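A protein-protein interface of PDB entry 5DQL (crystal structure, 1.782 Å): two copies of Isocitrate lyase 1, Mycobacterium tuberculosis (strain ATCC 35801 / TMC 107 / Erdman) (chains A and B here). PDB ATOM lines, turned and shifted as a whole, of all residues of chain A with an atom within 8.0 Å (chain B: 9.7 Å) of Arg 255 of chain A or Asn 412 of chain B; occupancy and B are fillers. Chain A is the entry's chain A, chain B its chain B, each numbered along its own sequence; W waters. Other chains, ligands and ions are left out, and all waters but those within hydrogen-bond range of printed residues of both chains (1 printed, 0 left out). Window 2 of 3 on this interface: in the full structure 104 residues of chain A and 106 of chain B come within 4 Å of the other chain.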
ATOM      1  N   LEU A 236     -21.711  -7.076 -13.556  1.00  0.00           N
ATOM      2  CA  LEU A 236     -21.530  -5.779 -12.912  1.00  0.00           C
ATOM      3  C   LEU A 236     -22.818  -4.963 -12.879  1.00  0.00           C
ATOM      4  O   LEU A 236     -23.697  -5.102 -13.754  1.00  0.00           O
ATOM      5  CB  LEU A 236     -20.449  -4.972 -13.630  1.00  0.00           C
ATOM      6  CG  LEU A 236     -19.066  -5.590 -13.794  1.00  0.00           C
ATOM      7  CD1 LEU A 236     -18.245  -4.794 -14.785  1.00  0.00           C
ATOM      8  CD2 LEU A 236     -18.360  -5.657 -12.453  1.00  0.00           C
ATOM      9  N   GLU A 252     -17.917  -7.143  -3.455  1.00  0.00           N
ATOM     10  CA  GLU A 252     -16.697  -6.799  -4.195  1.00  0.00           C
ATOM     11  C   GLU A 252     -16.922  -5.689  -5.235  1.00  0.00           C
ATOM     12  O   GLU A 252     -17.959  -5.649  -5.909  1.00  0.00           O
ATOM     13  CB  GLU A 252     -16.123  -8.034  -4.895  1.00  0.00           C
ATOM     14  CG  GLU A 252     -15.709  -9.148  -3.947  1.00  0.00           C
ATOM     15  CD  GLU A 252     -14.836 -10.195  -4.624  1.00  0.00           C
ATOM     16  OE1 GLU A 252     -15.004 -10.406  -5.851  1.00  0.00           O
ATOM     17  OE2 GLU A 252     -13.980 -10.801  -3.930  1.00  0.00           O
ATOM     18  N   ARG A 253     -15.944  -4.799  -5.366  1.00  0.00           N
ATOM     19  CA  ARG A 253     -16.038  -3.703  -6.320  1.00  0.00           C
ATOM     20  C   ARG A 253     -14.867  -3.680  -7.309  1.00  0.00           C
ATOM     21  O   ARG A 253     -13.795  -4.223  -7.033  1.00  0.00           O
ATOM     22  CB  ARG A 253     -16.156  -2.360  -5.593  1.00  0.00           C
ATOM     23  CG  ARG A 253     -17.505  -2.137  -4.923  1.00  0.00           C
ATOM     24  CD  ARG A 253     -18.105  -0.796  -5.319  1.00  0.00           C
ATOM     25  NE  ARG A 253     -17.993   0.195  -4.254  1.00  0.00           N
ATOM     26  CZ  ARG A 253     -17.953   1.509  -4.453  1.00  0.00           C
ATOM     27  NH1 ARG A 253     -18.003   2.002  -5.687  1.00  0.00           N
ATOM     28  NH2 ARG A 253     -17.851   2.334  -3.419  1.00  0.00           N
ATOM     29  N   THR A 254     -15.097  -3.069  -8.471  1.00  0.00           N
ATOM     30  CA  THR A 254     -14.049  -2.845  -9.462  1.00  0.00           C
ATOM     31  C   THR A 254     -13.432  -1.461  -9.236  1.00  0.00           C
ATOM     32  O   THR A 254     -13.965  -0.661  -8.469  1.00  0.00           O
ATOM     33  CB  THR A 254     -14.622  -2.918 -10.888  1.00  0.00           C
ATOM     34  OG1 THR A 254     -15.339  -1.710 -11.185  1.00  0.00           O
ATOM     35  CG2 THR A 254     -15.561  -4.088 -11.006  1.00  0.00           C
ATOM     36  N   ARG A 255     -12.321  -1.179  -9.914  1.00  0.00           N
ATOM     37  CA  ARG A 255     -11.632   0.102  -9.760  1.00  0.00           C
ATOM     38  C   ARG A 255     -12.447   1.291 -10.235  1.00  0.00           C
ATOM     39  O   ARG A 255     -12.246   2.410  -9.766  1.00  0.00           O
ATOM     40  CB  ARG A 255     -10.304   0.082 -10.499  1.00  0.00           C
ATOM     41  CG  ARG A 255      -9.377  -0.982  -9.990  1.00  0.00           C
ATOM     42  CD  ARG A 255      -8.002  -0.900 -10.609  1.00  0.00           C
ATOM     43  NE  ARG A 255      -7.141  -1.919 -10.022  1.00  0.00           N
ATOM     44  CZ  ARG A 255      -7.180  -3.208 -10.351  1.00  0.00           C
ATOM     45  NH1 ARG A 255      -8.032  -3.638 -11.272  1.00  0.00           N
ATOM     46  NH2 ARG A 255      -6.366  -4.070  -9.757  1.00  0.00           N
ATOM     47  N   GLU A 256     -13.357   1.056 -11.173  1.00  0.00           N
ATOM     48  CA  GLU A 256     -14.220   2.128 -11.667  1.00  0.00           C
ATOM     49  C   GLU A 256     -15.323   2.435 -10.664  1.00  0.00           C
ATOM     50  O   GLU A 256     -15.942   3.499 -10.713  1.00  0.00           O
ATOM     51  CB  GLU A 256     -14.846   1.759 -13.016  1.00  0.00           C
ATOM     52  CG  GLU A 256     -13.847   1.372 -14.088  1.00  0.00           C
ATOM     53  CD  GLU A 256     -13.784  -0.130 -14.294  1.00  0.00           C
ATOM     54  OE1 GLU A 256     -14.007  -0.873 -13.314  1.00  0.00           O
ATOM     55  OE2 GLU A 256     -13.526  -0.563 -15.439  1.00  0.00           O
ATOM     56  N   GLY A 257     -15.575   1.491  -9.761  1.00  0.00           N
ATOM     57  CA  GLY A 257     -16.593   1.688  -8.742  1.00  0.00           C
ATOM     58  C   GLY A 257     -17.811   0.807  -8.940  1.00  0.00           C
ATOM     59  O   GLY A 257     -18.775   0.896  -8.178  1.00  0.00           O
ATOM     60  N   PHE A 258     -17.771  -0.037  -9.970  1.00  0.00           N
ATOM     61  CA  PHE A 258     -18.884  -0.934 -10.270  1.00  0.00           C
ATOM     62  C   PHE A 258     -19.016  -2.015  -9.192  1.00  0.00           C
ATOM     63  O   PHE A 258     -18.015  -2.435  -8.606  1.00  0.00           O
ATOM     64  CB  PHE A 258     -18.674  -1.583 -11.645  1.00  0.00           C
ATOM     65  CG  PHE A 258     -18.674  -0.597 -12.802  1.00  0.00           C
ATOM     66  CD1 PHE A 258     -19.673   0.357 -12.921  1.00  0.00           C
ATOM     67  CD2 PHE A 258     -17.672  -0.641 -13.782  1.00  0.00           C
ATOM     68  CE1 PHE A 258     -19.674   1.263 -13.994  1.00  0.00           C
ATOM     69  CE2 PHE A 258     -17.666   0.266 -14.863  1.00  0.00           C
ATOM     70  CZ  PHE A 258     -18.672   1.209 -14.962  1.00  0.00           C
ATOM     71  N   ARG A 260     -19.854  -5.896  -8.299  1.00  0.00           N
ATOM     72  CA  ARG A 260     -19.997  -7.230  -8.850  1.00  0.00           C
ATOM     73  C   ARG A 260     -21.329  -7.803  -8.384  1.00  0.00           C
ATOM     74  O   ARG A 260     -21.795  -7.507  -7.276  1.00  0.00           O
ATOM     75  CB  ARG A 260     -18.835  -8.104  -8.412  1.00  0.00           C
ATOM     76  CG  ARG A 260     -17.501  -7.526  -8.830  1.00  0.00           C
ATOM     77  CD  ARG A 260     -16.379  -8.559  -8.859  1.00  0.00           C
ATOM     78  NE  ARG A 260     -15.083  -7.933  -9.135  1.00  0.00           N
ATOM     79  CZ  ARG A 260     -14.668  -7.559 -10.346  1.00  0.00           C
ATOM     80  NH1 ARG A 260     -15.448  -7.752 -11.412  1.00  0.00           N
ATOM     81  NH2 ARG A 260     -13.470  -6.993 -10.493  1.00  0.00           N
ATOM     82  N   ASP B 403     -11.759  -2.624 -28.209  1.00  0.00           N
ATOM     83  CA  ASP B 403     -11.218  -3.126 -26.946  1.00  0.00           C
ATOM     84  C   ASP B 403      -9.795  -2.625 -26.789  1.00  0.00           C
ATOM     85  O   ASP B 403      -9.339  -2.355 -25.678  1.00  0.00           O
ATOM     86  CB  ASP B 403     -11.216  -4.664 -26.889  1.00  0.00           C
ATOM     87  CG  ASP B 403     -12.543  -5.244 -26.429  1.00  0.00           C
ATOM     88  OD1 ASP B 403     -13.440  -4.463 -26.031  1.00  0.00           O
ATOM     89  OD2 ASP B 403     -12.675  -6.492 -26.463  1.00  0.00           O
ATOM     90  N   ILE B 405      -8.487   0.221 -28.090  1.00  0.00           N
ATOM     91  CA  ILE B 405      -8.562   1.611 -27.630  1.00  0.00           C
ATOM     92  C   ILE B 405      -8.853   1.646 -26.133  1.00  0.00           C
ATOM     93  O   ILE B 405      -8.210   2.394 -25.380  1.00  0.00           O
ATOM     94  CB  ILE B 405      -9.614   2.438 -28.424  1.00  0.00           C
ATOM     95  CG1 ILE B 405      -9.099   2.672 -29.848  1.00  0.00           C
ATOM     96  CG2 ILE B 405      -9.886   3.765 -27.713  1.00  0.00           C
ATOM     97  CD1 ILE B 405     -10.160   2.993 -30.885  1.00  0.00           C
ATOM     98  N   ALA B 406      -9.796   0.810 -25.696  1.00  0.00           N
ATOM     99  CA  ALA B 406     -10.260   0.841 -24.310  1.00  0.00           C
ATOM    100  C   ALA B 406      -9.127   0.499 -23.342  1.00  0.00           C
ATOM    101  O   ALA B 406      -8.938   1.171 -22.323  1.00  0.00           O
ATOM    102  CB  ALA B 406     -11.434  -0.113 -24.119  1.00  0.00           C
ATOM    103  N   THR B 407      -8.365  -0.543 -23.669  1.00  0.00           N
ATOM    104  CA  THR B 407      -7.253  -0.948 -22.810  1.00  0.00           C
ATOM    105  C   THR B 407      -6.028  -0.030 -22.932  1.00  0.00           C
ATOM    106  O   THR B 407      -5.200   0.028 -22.021  1.00  0.00           O
ATOM    107  CB  THR B 407      -6.877  -2.441 -22.977  1.00  0.00           C
ATOM    108  OG1 THR B 407      -6.545  -2.711 -24.338  1.00  0.00           O
ATOM    109  CG2 THR B 407      -8.046  -3.326 -22.580  1.00  0.00           C
ATOM    110  N   THR B 408      -5.930   0.706 -24.041  1.00  0.00           N
ATOM    111  CA  THR B 408      -4.887   1.719 -24.205  1.00  0.00           C
ATOM    112  C   THR B 408      -5.125   2.917 -23.287  1.00  0.00           C
ATOM    113  O   THR B 408      -4.184   3.466 -22.691  1.00  0.00           O
ATOM    114  CB  THR B 408      -4.784   2.192 -25.668  1.00  0.00           C
ATOM    115  OG1 THR B 408      -4.438   1.075 -26.506  1.00  0.00           O
ATOM    116  CG2 THR B 408      -3.726   3.249 -25.805  1.00  0.00           C
ATOM    117  N   VAL B 409      -6.391   3.318 -23.183  1.00  0.00           N
ATOM    118  CA  VAL B 409      -6.818   4.361 -22.251  1.00  0.00           C
ATOM    119  C   VAL B 409      -6.766   3.887 -20.792  1.00  0.00           C
ATOM    120  O   VAL B 409      -6.301   4.611 -19.916  1.00  0.00           O
ATOM    121  CB  VAL B 409      -8.239   4.857 -22.601  1.00  0.00           C
ATOM    122  CG1 VAL B 409      -8.704   5.874 -21.589  1.00  0.00           C
ATOM    123  CG2 VAL B 409      -8.235   5.483 -23.983  1.00  0.00           C
ATOM    124  N   ASP B 410      -7.232   2.658 -20.555  1.00  0.00           N
ATOM    125  CA  ASP B 410      -7.310   2.080 -19.212  1.00  0.00           C
ATOM    126  C   ASP B 410      -7.033   0.574 -19.254  1.00  0.00           C
ATOM    127  O   ASP B 410      -7.952  -0.227 -19.472  1.00  0.00           O
ATOM    128  CB  ASP B 410      -8.699   2.347 -18.608  1.00  0.00           C
ATOM    129  CG  ASP B 410      -8.874   1.726 -17.223  1.00  0.00           C
ATOM    130  OD1 ASP B 410      -7.854   1.400 -16.569  1.00  0.00           O
ATOM    131  OD2 ASP B 410     -10.045   1.567 -16.790  1.00  0.00           O
ATOM    132  N   PRO B 411      -5.765   0.180 -19.035  1.00  0.00           N
ATOM    133  CA  PRO B 411      -5.395  -1.245 -19.097  1.00  0.00           C
ATOM    134  C   PRO B 411      -6.201  -2.116 -18.126  1.00  0.00           C
ATOM    135  O   PRO B 411      -6.362  -3.311 -18.380  1.00  0.00           O
ATOM    136  CB  PRO B 411      -3.905  -1.242 -18.719  1.00  0.00           C
ATOM    137  CG  PRO B 411      -3.425   0.147 -19.083  1.00  0.00           C
ATOM    138  CD  PRO B 411      -4.607   1.045 -18.748  1.00  0.00           C
ATOM    139  N   ASN B 412      -6.697  -1.528 -17.043  1.00  0.00           N
ATOM    140  CA  ASN B 412      -7.468  -2.268 -16.045  1.00  0.00           C
ATOM    141  C   ASN B 412      -8.976  -2.259 -16.270  1.00  0.00           C
ATOM    142  O   ASN B 412      -9.734  -2.637 -15.374  1.00  0.00           O
ATOM    143  CB  ASN B 412      -7.152  -1.753 -14.633  1.00  0.00           C
ATOM    144  CG  ASN B 412      -5.680  -1.881 -14.296  1.00  0.00           C
ATOM    145  OD1 ASN B 412      -5.013  -2.820 -14.738  1.00  0.00           O
ATOM    146  ND2 ASN B 412      -5.155  -0.921 -13.542  1.00  0.00           N
ATOM    147  N   SER B 413      -9.415  -1.845 -17.460  1.00  0.00           N
ATOM    148  CA  SER B 413     -10.856  -1.729 -17.714  1.00  0.00           C
ATOM    149  C   SER B 413     -11.619  -3.023 -17.456  1.00  0.00           C
ATOM    150  O   SER B 413     -11.224  -4.104 -17.925  1.00  0.00           O
ATOM    151  CB  SER B 413     -11.147  -1.274 -19.134  1.00  0.00           C
ATOM    152  OG  SER B 413     -12.528  -1.419 -19.386  1.00  0.00           O
ATOM    153  N   SER B 414     -12.718  -2.896 -16.718  1.00  0.00           N
ATOM    154  CA  SER B 414     -13.594  -4.021 -16.399  1.00  0.00           C
ATOM    155  C   SER B 414     -14.673  -4.245 -17.453  1.00  0.00           C
ATOM    156  O   SER B 414     -15.517  -5.130 -17.302  1.00  0.00           O
ATOM    157  CB  SER B 414     -14.289  -3.767 -15.061  1.00  0.00           C
ATOM    158  OG  SER B 414     -13.366  -3.314 -14.101  1.00  0.00           O
ATOM    159  N   THR B 415     -14.669  -3.434 -18.506  1.00  0.00           N
ATOM    160  CA  THR B 415     -15.815  -3.395 -19.399  1.00  0.00           C
ATOM    161  C   THR B 415     -15.460  -3.578 -20.876  1.00  0.00           C
ATOM    162  O   THR B 415     -16.132  -3.026 -21.742  1.00  0.00           O
ATOM    163  CB  THR B 415     -16.620  -2.100 -19.209  1.00  0.00           C
ATOM    164  OG1 THR B 415     -15.761  -0.972 -19.416  1.00  0.00           O
ATOM    165  CG2 THR B 415     -17.194  -2.035 -17.799  1.00  0.00           C
ATOM    166  N   THR B 416     -14.412  -4.353 -21.159  1.00  0.00           N
ATOM    167  CA  THR B 416     -14.072  -4.676 -22.545  1.00  0.00           C
ATOM    168  C   THR B 416     -15.026  -5.753 -23.079  1.00  0.00           C
ATOM    169  O   THR B 416     -15.642  -6.476 -22.286  1.00  0.00           O
ATOM    170  CB  THR B 416     -12.602  -5.098 -22.691  1.00  0.00           C
ATOM    171  OG1 THR B 416     -12.383  -6.356 -22.026  1.00  0.00           O
ATOM    172  CG2 THR B 416     -11.701  -4.030 -22.106  1.00  0.00           C
HETATM  173  O   HOH W   1     -14.582   1.054 -17.492  1.00  0.00           O
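The side-chain carboxylate (OE1) of Glu 256 of chain A is in hydrogen-bond range of the side-chain hydroxyl (OG) of Ser 414 of chain B (2.6 Å).
Water W1 lies within hydrogen-bond range of the side-chain carboxylate of Glu 256 of chain A (2.8 Å) and the side-chain hydroxyl of Thr 415 of chain B (3.0 Å).
Among the printed residues, pairs that only touch across the chains: Leu 236 of chain A with Ser 414 of chain B (3.7 Å), Thr 254 of chain A with Ser 414 of chain B (3.5 Å), Arg 255 of chain A with Asn 412 of chain B (3.95 Å), Glu 256 of chain A with Ser 413 of chain B (3.7 Å) and Phe 258 of chain A with Thr 415 of chain B (3.8 Å).
No position is printed for both chains.
The side-chain hydroxyl of Ser 413 of chain B lies within hydrogen-bond range of the backbone NH of Thr 415 of chain B, at 3.1 Å. OG1 of Thr 254 of chain A sits at hydrogen-bond distance from N of Phe 258 of chain A (3.2 Å). The side-chain carboxylate (OE1) of Glu 256 of chain A lies within hydrogen-bond range of the side-chain hydroxyl (OG1) of Thr 254 of chain A (2.6 Å). N of Asn 412 of chain B lies close to OD1 of Asp 410 of chain B (3.2 Å).
Of the 9 printed residues of chain A, 5 touch a printed residue of chain B. Hydrophobic or aromatic side chains of chain A within 4 Å of the printed part of chain B: Leu 236 and Phe 258. Of the 13 printed residues of chain B, 4 touch a printed residue of chain A. Printed residues of chain B that touch a printed residue of chain A: Asn 412, Ser 413, Ser 414 and Thr 415. Among the printed residues, no Asp or Glu carboxylate lies within 4 Å of a Lys or Arg side-chain nitrogen of the other chain.
Arg 255 of chain A touches just one residue of chain B: Asn 412 (3.95 Å). Of chain A, only Arg 255 (3.95 Å) comes within 4 Å of Asn 412 of chain B. Of chain B, only Ser 413 (3.7 Å) and Ser 414 (2.6 Å) come within 4 Å of Glu 256 of chain A. Of the printed residues of chain A, Ser 413 of chain B touches Glu 256. Of the printed residues of chain A, Ser 414 of chain B touches Leu 236 (3.7 Å), Thr 254 (3.5 Å) and Glu 256 (2.6 Å). Of the printed residues of chain A, Thr 415 of chain B touches Phe 258 (3.8 Å). Printed residues of chain B within 4 Å of Leu 236 of chain A: Ser 414 (3.7 Å). Gly 257 of chain A touches none of the printed residues of chain B. The nearest residue of chain A that does not touch Asn 412 of chain B is Glu 256 of chain A (4.3 Å).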
